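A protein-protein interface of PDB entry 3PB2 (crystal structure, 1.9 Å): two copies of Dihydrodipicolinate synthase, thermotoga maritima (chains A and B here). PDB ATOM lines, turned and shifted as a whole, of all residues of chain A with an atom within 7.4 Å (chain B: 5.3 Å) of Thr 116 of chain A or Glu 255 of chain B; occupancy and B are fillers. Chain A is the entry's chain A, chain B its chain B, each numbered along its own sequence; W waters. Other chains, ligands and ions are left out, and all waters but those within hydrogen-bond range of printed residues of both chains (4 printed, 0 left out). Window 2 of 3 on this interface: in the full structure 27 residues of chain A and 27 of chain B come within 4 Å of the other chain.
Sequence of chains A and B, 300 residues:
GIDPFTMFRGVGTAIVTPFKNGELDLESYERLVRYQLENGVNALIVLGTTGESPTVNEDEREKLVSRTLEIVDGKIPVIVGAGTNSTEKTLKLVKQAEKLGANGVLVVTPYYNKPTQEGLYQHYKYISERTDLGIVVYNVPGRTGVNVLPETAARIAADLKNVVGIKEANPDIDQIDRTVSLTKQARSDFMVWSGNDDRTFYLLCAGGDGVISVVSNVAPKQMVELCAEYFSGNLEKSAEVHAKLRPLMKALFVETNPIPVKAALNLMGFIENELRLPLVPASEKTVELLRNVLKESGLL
Of the printed residues of chain B, Lys 114 of chain A touches Thr 256 (2.6 Å).
Thr 116 of chain A touches just these residues of chain B: Glu 255 (3.9 Å), Ile 259 (3.7 Å) and Val 280 (3.6 Å).
Of the printed residues of chain B, Gly 119 of chain A touches Pro 278 (3.2 Å).
Of the printed residues of chain A, Glu 255 of chain B touches Thr 116.
Of the printed residues of chain A, Ile 259 of chain B touches Thr 116.
Of the printed residues of chain A, Val 280 of chain B touches Thr 116.
Thr 286 of chain B touches none of the printed residues of chain A.
The nearest residue of chain B that does not touch Thr 116 of chain A is Pro 278 of chain B (4.9 Å).
The nearest residue of chain A that does not touch Glu 255 of chain B is Lys 114 of chain A (6.5 Å).
The nearest printed residue of chain A that does not touch Val 280 of chain B is Gly 119 of chain A (4.2 Å).
No position is printed for both chains.
Among the printed residues, merely in contact across the chains: Asn 113 of chain A with Thr 256 of chain B, Asn 113 of chain A with Pro 278 of chain B, Pro 115 of chain A with Pro 278 of chain B, Thr 116 of chain A with Glu 255 of chain B, Thr 116 of chain A with Ile 259 of chain B, Thr 116 of chain A with Val 280 of chain B and Gly 119 of chain A with Pro 278 of chain B.
Water W2 bridges OG1 of Thr 256 of chain B (2.7 Å) and NZ of Lys 114 of chain A (3.5 Å).
Water W4 bridges the backbone carbonyl oxygen (O) of Asn 113 of chain A (2.7 Å) and the backbone carbonyl oxygen (O) of Asn 257 of chain B (2.7 Å).
Water W1 lies within hydrogen-bond range of the backbone carbonyl oxygen (O) of Pro 278 of chain B (2.8 Å), the side-chain hydroxyl (OG1) of Thr 116 of chain A (2.8 Å) and the backbone NH (N) of Val 280 of chain B (3.4 Å).
Water W3 lies within hydrogen-bond range of OG1 of Thr 256 of chain B (3.0 Å), O of Lys 114 of chain A (3.1 Å) and O of Pro 115 of chain A (3.1 Å).
The backbone carbonyl oxygen of Lys 114 of chain A lies within hydrogen-bond range of the side-chain hydroxyl of Thr 256 of chain B, at 2.6 Å.
N of Gly 119 of chain A lies within hydrogen-bond range of OG1 of Thr 116 of chain A.
The side-chain carboxylate (OE2) of Glu 255 of chain B is in hydrogen-bond range of the backbone NH (N) of Ser 283 of chain B, 2.9 Å away.
OE2 of Glu 255 of chain B sits at hydrogen-bond distance from OG1 of Thr 286 of chain B, at 2.6 Å.
Along chain A the printed residues that touch a printed residue of chain B span positions 113 to 119.
Printed residues of chain B that touch a printed residue of chain A: Glu 255, Thr 256, Ile 259, Pro 278 and Val 280.
Hydrophobic or aromatic side chains of chain B within 4 Å of the printed part of chain A: Ile 259, Pro 278 and Val 280.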
ATOM      1  N   ASN A 113       2.449  -0.968 -33.316  1.00  0.00           N
ATOM      2  CA  ASN A 113       3.253  -2.196 -33.477  1.00  0.00           C
ATOM      3  C   ASN A 113       3.225  -3.205 -32.315  1.00  0.00           C
ATOM      4  O   ASN A 113       3.844  -4.280 -32.399  1.00  0.00           O
ATOM      5  CB  ASN A 113       4.698  -1.936 -34.002  1.00  0.00           C
ATOM      6  CG  ASN A 113       5.490  -0.919 -33.172  1.00  0.00           C
ATOM      7  OD1 ASN A 113       5.065  -0.466 -32.113  1.00  0.00           O
ATOM      8  ND2 ASN A 113       6.679  -0.572 -33.670  1.00  0.00           N
ATOM      9  N   LYS A 114       2.498  -2.878 -31.247  1.00  0.00           N
ATOM     10  CA  LYS A 114       2.286  -3.818 -30.121  1.00  0.00           C
ATOM     11  C   LYS A 114       3.520  -4.597 -29.610  1.00  0.00           C
ATOM     12  O   LYS A 114       3.530  -5.821 -29.573  1.00  0.00           O
ATOM     13  CB  LYS A 114       1.156  -4.815 -30.459  1.00  0.00           C
ATOM     14  CG  LYS A 114      -0.197  -4.157 -30.772  1.00  0.00           C
ATOM     15  CD  LYS A 114      -1.354  -5.182 -30.755  1.00  0.00           C
ATOM     16  CE  LYS A 114      -1.186  -6.208 -31.868  1.00  0.00           C
ATOM     17  NZ  LYS A 114      -2.192  -7.319 -31.789  1.00  0.00           N
ATOM     18  N   PRO A 115       4.558  -3.883 -29.163  1.00  0.00           N
ATOM     19  CA  PRO A 115       5.756  -4.574 -28.673  1.00  0.00           C
ATOM     20  C   PRO A 115       5.464  -5.407 -27.433  1.00  0.00           C
ATOM     21  O   PRO A 115       4.535  -5.096 -26.665  1.00  0.00           O
ATOM     22  CB  PRO A 115       6.726  -3.425 -28.335  1.00  0.00           C
ATOM     23  CG  PRO A 115       5.846  -2.216 -28.157  1.00  0.00           C
ATOM     24  CD  PRO A 115       4.626  -2.427 -29.019  1.00  0.00           C
ATOM     25  N   THR A 116       6.234  -6.479 -27.269  1.00  0.00           N
ATOM     26  CA  THR A 116       6.222  -7.281 -26.056  1.00  0.00           C
ATOM     27  C   THR A 116       6.683  -6.441 -24.864  1.00  0.00           C
ATOM     28  O   THR A 116       7.229  -5.342 -25.038  1.00  0.00           O
ATOM     29  CB  THR A 116       7.170  -8.498 -26.202  1.00  0.00           C
ATOM     30  OG1 THR A 116       8.531  -8.044 -26.323  1.00  0.00           O
ATOM     31  CG2 THR A 116       6.818  -9.257 -27.459  1.00  0.00           C
ATOM     32  N   GLN A 117       6.470  -6.961 -23.657  1.00  0.00           N
ATOM     33  CA  GLN A 117       6.935  -6.290 -22.443  1.00  0.00           C
ATOM     34  C   GLN A 117       8.452  -6.095 -22.437  1.00  0.00           C
ATOM     35  O   GLN A 117       8.940  -5.038 -22.044  1.00  0.00           O
ATOM     36  CB  GLN A 117       6.487  -7.052 -21.189  1.00  0.00           C
ATOM     37  CG  GLN A 117       4.969  -7.176 -21.044  1.00  0.00           C
ATOM     38  CD  GLN A 117       4.295  -5.826 -20.906  1.00  0.00           C
ATOM     39  OE1 GLN A 117       4.506  -5.101 -19.921  1.00  0.00           O
ATOM     40  NE2 GLN A 117       3.472  -5.472 -21.896  1.00  0.00           N
ATOM     41  N   GLU A 118       9.198  -7.105 -22.874  1.00  0.00           N
ATOM     42  CA  GLU A 118      10.660  -6.969 -22.947  1.00  0.00           C
ATOM     43  C   GLU A 118      11.016  -5.880 -23.960  1.00  0.00           C
ATOM     44  O   GLU A 118      11.958  -5.119 -23.756  1.00  0.00           O
ATOM     45  CB  GLU A 118      11.327  -8.294 -23.310  1.00  0.00           C
ATOM     46  CG  GLU A 118      12.841  -8.215 -23.567  1.00  0.00           C
ATOM     47  CD  GLU A 118      13.654  -7.884 -22.322  1.00  0.00           C
ATOM     48  OE1 GLU A 118      13.118  -8.001 -21.210  1.00  0.00           O
ATOM     49  OE2 GLU A 118      14.837  -7.508 -22.458  1.00  0.00           O
ATOM     50  N   GLY A 119      10.237  -5.798 -25.039  1.00  0.00           N
ATOM     51  CA  GLY A 119      10.423  -4.760 -26.040  1.00  0.00           C
ATOM     52  C   GLY A 119      10.218  -3.372 -25.448  1.00  0.00           C
ATOM     53  O   GLY A 119      11.013  -2.463 -25.681  1.00  0.00           O
ATOM     54  N   LEU A 120       9.148  -3.204 -24.682  1.00  0.00           N
ATOM     55  CA  LEU A 120       8.907  -1.934 -23.986  1.00  0.00           C
ATOM     56  C   LEU A 120      10.095  -1.573 -23.096  1.00  0.00           C
ATOM     57  O   LEU A 120      10.542  -0.433 -23.065  1.00  0.00           O
ATOM     58  CB  LEU A 120       7.636  -2.025 -23.137  1.00  0.00           C
ATOM     59  CG  LEU A 120       6.338  -2.085 -23.961  1.00  0.00           C
ATOM     60  CD1 LEU A 120       5.126  -2.280 -23.047  1.00  0.00           C
ATOM     61  CD2 LEU A 120       6.205  -0.782 -24.756  1.00  0.00           C
ATOM     62  N   TYR A 121      10.585  -2.551 -22.345  1.00  0.00           N
ATOM     63  CA  TYR A 121      11.710  -2.310 -21.458  1.00  0.00           C
ATOM     64  C   TYR A 121      12.939  -1.840 -22.244  1.00  0.00           C
ATOM     65  O   TYR A 121      13.581  -0.850 -21.889  1.00  0.00           O
ATOM     66  CB  TYR A 121      12.039  -3.584 -20.672  1.00  0.00           C
ATOM     67  CG  TYR A 121      13.257  -3.435 -19.799  1.00  0.00           C
ATOM     68  CD1 TYR A 121      13.178  -2.787 -18.568  1.00  0.00           C
ATOM     69  CD2 TYR A 121      14.489  -3.936 -20.202  1.00  0.00           C
ATOM     70  CE1 TYR A 121      14.303  -2.642 -17.755  1.00  0.00           C
ATOM     71  CE2 TYR A 121      15.620  -3.798 -19.388  1.00  0.00           C
ATOM     72  CZ  TYR A 121      15.521  -3.148 -18.179  1.00  0.00           C
ATOM     73  OH  TYR A 121      16.638  -3.012 -17.380  1.00  0.00           O
ATOM     74  N   GLN A 122      13.259  -2.547 -23.320  1.00  0.00           N
ATOM     75  CA  GLN A 122      14.438  -2.205 -24.116  1.00  0.00           C
ATOM     76  C   GLN A 122      14.287  -0.838 -24.772  1.00  0.00           C
ATOM     77  O   GLN A 122      15.259  -0.125 -24.938  1.00  0.00           O
ATOM     78  CB  GLN A 122      14.714  -3.278 -25.169  1.00  0.00           C
ATOM     79  CG  GLN A 122      15.157  -4.624 -24.557  1.00  0.00           C
ATOM     80  CD  GLN A 122      16.492  -4.503 -23.842  1.00  0.00           C
ATOM     81  OE1 GLN A 122      17.277  -3.592 -24.120  1.00  0.00           O
ATOM     82  NE2 GLN A 122      16.758  -5.417 -22.917  1.00  0.00           N
ATOM     83  N   VAL A 146      -1.346  -1.412 -26.660  1.00  0.00           N
ATOM     84  CA  VAL A 146      -0.473  -2.172 -25.750  1.00  0.00           C
ATOM     85  C   VAL A 146      -0.591  -1.646 -24.326  1.00  0.00           C
ATOM     86  O   VAL A 146      -0.773  -0.445 -24.105  1.00  0.00           O
ATOM     87  CB  VAL A 146       1.009  -2.132 -26.215  1.00  0.00           C
ATOM     88  CG1 VAL A 146       1.597  -0.731 -26.028  1.00  0.00           C
ATOM     89  CG2 VAL A 146       1.861  -3.170 -25.469  1.00  0.00           C
ATOM     90  N   ASN A 147      -0.473  -2.540 -23.352  1.00  0.00           N
ATOM     91  CA  ASN A 147      -0.520  -2.146 -21.942  1.00  0.00           C
ATOM     92  C   ASN A 147       0.782  -2.486 -21.225  1.00  0.00           C
ATOM     93  O   ASN A 147       1.228  -3.640 -21.248  1.00  0.00           O
ATOM     94  CB  ASN A 147      -1.685  -2.837 -21.220  1.00  0.00           C
ATOM     95  CG  ASN A 147      -1.827  -2.396 -19.772  1.00  0.00           C
ATOM     96  OD1 ASN A 147      -1.972  -1.202 -19.483  1.00  0.00           O
ATOM     97  ND2 ASN A 147      -1.838  -3.358 -18.858  1.00  0.00           N
ATOM     98  N   THR A 152       6.258  -4.582 -15.285  1.00  0.00           N
ATOM     99  CA  THR A 152       7.196  -4.031 -16.259  1.00  0.00           C
ATOM    100  C   THR A 152       7.514  -2.593 -15.871  1.00  0.00           C
ATOM    101  O   THR A 152       8.669  -2.155 -15.940  1.00  0.00           O
ATOM    102  CB  THR A 152       6.614  -4.076 -17.700  1.00  0.00           C
ATOM    103  OG1 THR A 152       6.290  -5.435 -18.054  1.00  0.00           O
ATOM    104  CG2 THR A 152       7.618  -3.507 -18.713  1.00  0.00           C
ATOM    105  N   ALA B 251      -0.319 -20.127 -34.348  1.00  0.00           N
ATOM    106  CA  ALA B 251       1.062 -20.023 -33.873  1.00  0.00           C
ATOM    107  C   ALA B 251       1.734 -18.706 -34.290  1.00  0.00           C
ATOM    108  O   ALA B 251       2.594 -18.180 -33.574  1.00  0.00           O
ATOM    109  CB  ALA B 251       1.869 -21.210 -34.354  1.00  0.00           C
ATOM    110  N   LEU B 252       1.343 -18.171 -35.442  1.00  0.00           N
ATOM    111  CA  LEU B 252       1.990 -16.976 -35.989  1.00  0.00           C
ATOM    112  C   LEU B 252       1.549 -15.707 -35.269  1.00  0.00           C
ATOM    113  O   LEU B 252       2.041 -14.622 -35.572  1.00  0.00           O
ATOM    114  CB  LEU B 252       1.764 -16.850 -37.503  1.00  0.00           C
ATOM    115  CG  LEU B 252       2.512 -17.888 -38.355  1.00  0.00           C
ATOM    116  CD1 LEU B 252       2.249 -17.667 -39.821  1.00  0.00           C
ATOM    117  CD2 LEU B 252       4.031 -17.865 -38.074  1.00  0.00           C
ATOM    118  N   PHE B 253       0.654 -15.849 -34.292  1.00  0.00           N
ATOM    119  CA  PHE B 253       0.232 -14.699 -33.496  1.00  0.00           C
ATOM    120  C   PHE B 253       0.318 -14.918 -31.994  1.00  0.00           C
ATOM    121  O   PHE B 253      -0.248 -14.149 -31.235  1.00  0.00           O
ATOM    122  CB  PHE B 253      -1.170 -14.248 -33.926  1.00  0.00           C
ATOM    123  CG  PHE B 253      -1.222 -13.854 -35.363  1.00  0.00           C
ATOM    124  CD1 PHE B 253      -0.940 -12.551 -35.742  1.00  0.00           C
ATOM    125  CD2 PHE B 253      -1.462 -14.804 -36.345  1.00  0.00           C
ATOM    126  CE1 PHE B 253      -0.942 -12.182 -37.081  1.00  0.00           C
ATOM    127  CE2 PHE B 253      -1.466 -14.449 -37.679  1.00  0.00           C
ATOM    128  CZ  PHE B 253      -1.203 -13.131 -38.047  1.00  0.00           C
ATOM    129  N   VAL B 254       1.041 -15.953 -31.567  1.00  0.00           N
ATOM    130  CA  VAL B 254       1.222 -16.168 -30.130  1.00  0.00           C
ATOM    131  C   VAL B 254       2.042 -15.044 -29.492  1.00  0.00           C
ATOM    132  O   VAL B 254       1.950 -14.807 -28.280  1.00  0.00           O
ATOM    133  CB  VAL B 254       1.817 -17.557 -29.763  1.00  0.00           C
ATOM    134  CG1 VAL B 254       0.881 -18.675 -30.191  1.00  0.00           C
ATOM    135  CG2 VAL B 254       3.227 -17.735 -30.345  1.00  0.00           C
ATOM    136  N   GLU B 255       2.864 -14.386 -30.304  1.00  0.00           N
ATOM    137  CA  GLU B 255       3.430 -13.092 -29.947  1.00  0.00           C
ATOM    138  C   GLU B 255       3.103 -12.147 -31.095  1.00  0.00           C
ATOM    139  O   GLU B 255       2.738 -12.599 -32.185  1.00  0.00           O
ATOM    140  CB  GLU B 255       4.946 -13.180 -29.772  1.00  0.00           C
ATOM    141  CG  GLU B 255       5.370 -14.146 -28.660  1.00  0.00           C
ATOM    142  CD  GLU B 255       6.877 -14.086 -28.420  1.00  0.00           C
ATOM    143  OE1 GLU B 255       7.366 -13.042 -27.959  1.00  0.00           O
ATOM    144  OE2 GLU B 255       7.572 -15.074 -28.708  1.00  0.00           O
ATOM    145  N   THR B 256       3.241 -10.843 -30.853  1.00  0.00           N
ATOM    146  CA  THR B 256       2.882  -9.836 -31.850  1.00  0.00           C
ATOM    147  C   THR B 256       3.553 -10.088 -33.201  1.00  0.00           C
ATOM    148  O   THR B 256       4.768 -10.189 -33.294  1.00  0.00           O
ATOM    149  CB  THR B 256       3.225  -8.423 -31.363  1.00  0.00           C
ATOM    150  OG1 THR B 256       2.480  -8.135 -30.168  1.00  0.00           O
ATOM    151  CG2 THR B 256       2.899  -7.384 -32.448  1.00  0.00           C
ATOM    152  N   ASN B 257       2.743 -10.174 -34.249  1.00  0.00           N
ATOM    153  CA  ASN B 257       3.247 -10.218 -35.625  1.00  0.00           C
ATOM    154  C   ASN B 257       4.041  -8.936 -35.927  1.00  0.00           C
ATOM    155  O   ASN B 257       3.593  -7.842 -35.579  1.00  0.00           O
ATOM    156  CB  ASN B 257       2.045 -10.365 -36.580  1.00  0.00           C
ATOM    157  CG  ASN B 257       2.448 -10.276 -38.041  1.00  0.00           C
ATOM    158  OD1 ASN B 257       3.257 -11.074 -38.525  1.00  0.00           O
ATOM    159  ND2 ASN B 257       1.915  -9.274 -38.744  1.00  0.00           N
ATOM    160  N   ILE B 259       6.782 -10.996 -35.055  1.00  0.00           N
ATOM    161  CA  ILE B 259       7.795 -11.698 -34.264  1.00  0.00           C
ATOM    162  C   ILE B 259       7.793 -13.215 -34.564  1.00  0.00           C
ATOM    163  O   ILE B 259       8.847 -13.794 -34.856  1.00  0.00           O
ATOM    164  CB  ILE B 259       7.712 -11.363 -32.740  1.00  0.00           C
ATOM    165  CG1 ILE B 259       8.102  -9.897 -32.484  1.00  0.00           C
ATOM    166  CG2 ILE B 259       8.609 -12.322 -31.887  1.00  0.00           C
ATOM    167  CD1 ILE B 259       7.784  -9.398 -31.041  1.00  0.00           C
ATOM    168  N   PRO B 260       6.611 -13.858 -34.545  1.00  0.00           N
ATOM    169  CA  PRO B 260       6.643 -15.292 -34.840  1.00  0.00           C
ATOM    170  C   PRO B 260       6.970 -15.594 -36.296  1.00  0.00           C
ATOM    171  O   PRO B 260       7.726 -16.528 -36.541  1.00  0.00           O
ATOM    172  CB  PRO B 260       5.220 -15.749 -34.504  1.00  0.00           C
ATOM    173  CG  PRO B 260       4.764 -14.781 -33.491  1.00  0.00           C
ATOM    174  CD  PRO B 260       5.337 -13.465 -33.916  1.00  0.00           C
ATOM    175  N   PRO B 278      11.005  -1.208 -31.193  1.00  0.00           N
ATOM    176  CA  PRO B 278      10.698  -1.964 -29.969  1.00  0.00           C
ATOM    177  C   PRO B 278      10.387  -3.462 -30.148  1.00  0.00           C
ATOM    178  O   PRO B 278      10.074  -4.134 -29.153  1.00  0.00           O
ATOM    179  CB  PRO B 278       9.453  -1.255 -29.425  1.00  0.00           C
ATOM    180  CG  PRO B 278       8.758  -0.740 -30.647  1.00  0.00           C
ATOM    181  CD  PRO B 278       9.888  -0.328 -31.587  1.00  0.00           C
ATOM    182  N   VAL B 280      11.446  -7.404 -30.658  1.00  0.00           N
ATOM    183  CA  VAL B 280      12.566  -8.279 -30.300  1.00  0.00           C
ATOM    184  C   VAL B 280      12.262  -9.702 -30.767  1.00  0.00           C
ATOM    185  O   VAL B 280      11.103 -10.035 -31.024  1.00  0.00           O
ATOM    186  CB  VAL B 280      12.858  -8.278 -28.767  1.00  0.00           C
ATOM    187  CG1 VAL B 280      13.250  -6.872 -28.281  1.00  0.00           C
ATOM    188  CG2 VAL B 280      11.663  -8.826 -27.983  1.00  0.00           C
ATOM    189  N   PRO B 281      13.297 -10.547 -30.903  1.00  0.00           N
ATOM    190  CA  PRO B 281      13.037 -11.915 -31.377  1.00  0.00           C
ATOM    191  C   PRO B 281      12.089 -12.717 -30.480  1.00  0.00           C
ATOM    192  O   PRO B 281      11.958 -12.440 -29.278  1.00  0.00           O
ATOM    193  CB  PRO B 281      14.429 -12.570 -31.362  1.00  0.00           C
ATOM    194  CG  PRO B 281      15.383 -11.403 -31.527  1.00  0.00           C
ATOM    195  CD  PRO B 281      14.732 -10.284 -30.723  1.00  0.00           C
ATOM    196  N   ALA B 282      11.467 -13.728 -31.078  1.00  0.00           N
ATOM    197  CA  ALA B 282      10.559 -14.629 -30.382  1.00  0.00           C
ATOM    198  C   ALA B 282      11.205 -15.365 -29.187  1.00  0.00           C
ATOM    199  O   ALA B 282      12.401 -15.653 -29.172  1.00  0.00           O
ATOM    200  CB  ALA B 282       9.954 -15.635 -31.379  1.00  0.00           C
ATOM    201  N   SER B 283      10.396 -15.660 -28.180  1.00  0.00           N
ATOM    202  CA  SER B 283      10.860 -16.447 -27.032  1.00  0.00           C
ATOM    203  C   SER B 283      11.145 -17.888 -27.453  1.00  0.00           C
ATOM    204  O   SER B 283      10.759 -18.305 -28.536  1.00  0.00           O
ATOM    205  CB  SER B 283       9.783 -16.465 -25.961  1.00  0.00           C
ATOM    206  OG  SER B 283       8.644 -17.177 -26.425  1.00  0.00           O
ATOM    207  N   THR B 286       7.878 -19.809 -28.121  1.00  0.00           N
ATOM    208  CA  THR B 286       7.346 -19.559 -29.447  1.00  0.00           C
ATOM    209  C   THR B 286       8.108 -20.307 -30.533  1.00  0.00           C
ATOM    210  O   THR B 286       7.501 -20.890 -31.422  1.00  0.00           O
ATOM    211  CB  THR B 286       7.352 -18.059 -29.741  1.00  0.00           C
ATOM    212  OG1 THR B 286       6.444 -17.432 -28.839  1.00  0.00           O
ATOM    213  CG2 THR B 286       6.932 -17.762 -31.190  1.00  0.00           C
HETATM  214  O   HOH W   1       8.745  -6.539 -28.699  1.00  0.00           O
HETATM  215  O   HOH W   2       0.005  -9.107 -29.786  1.00  0.00           O
HETATM  216  O   HOH W   3       2.619  -7.521 -27.188  1.00  0.00           O
HETATM  217  O   HOH W   4       4.075  -5.213 -34.952  1.00  0.00           O
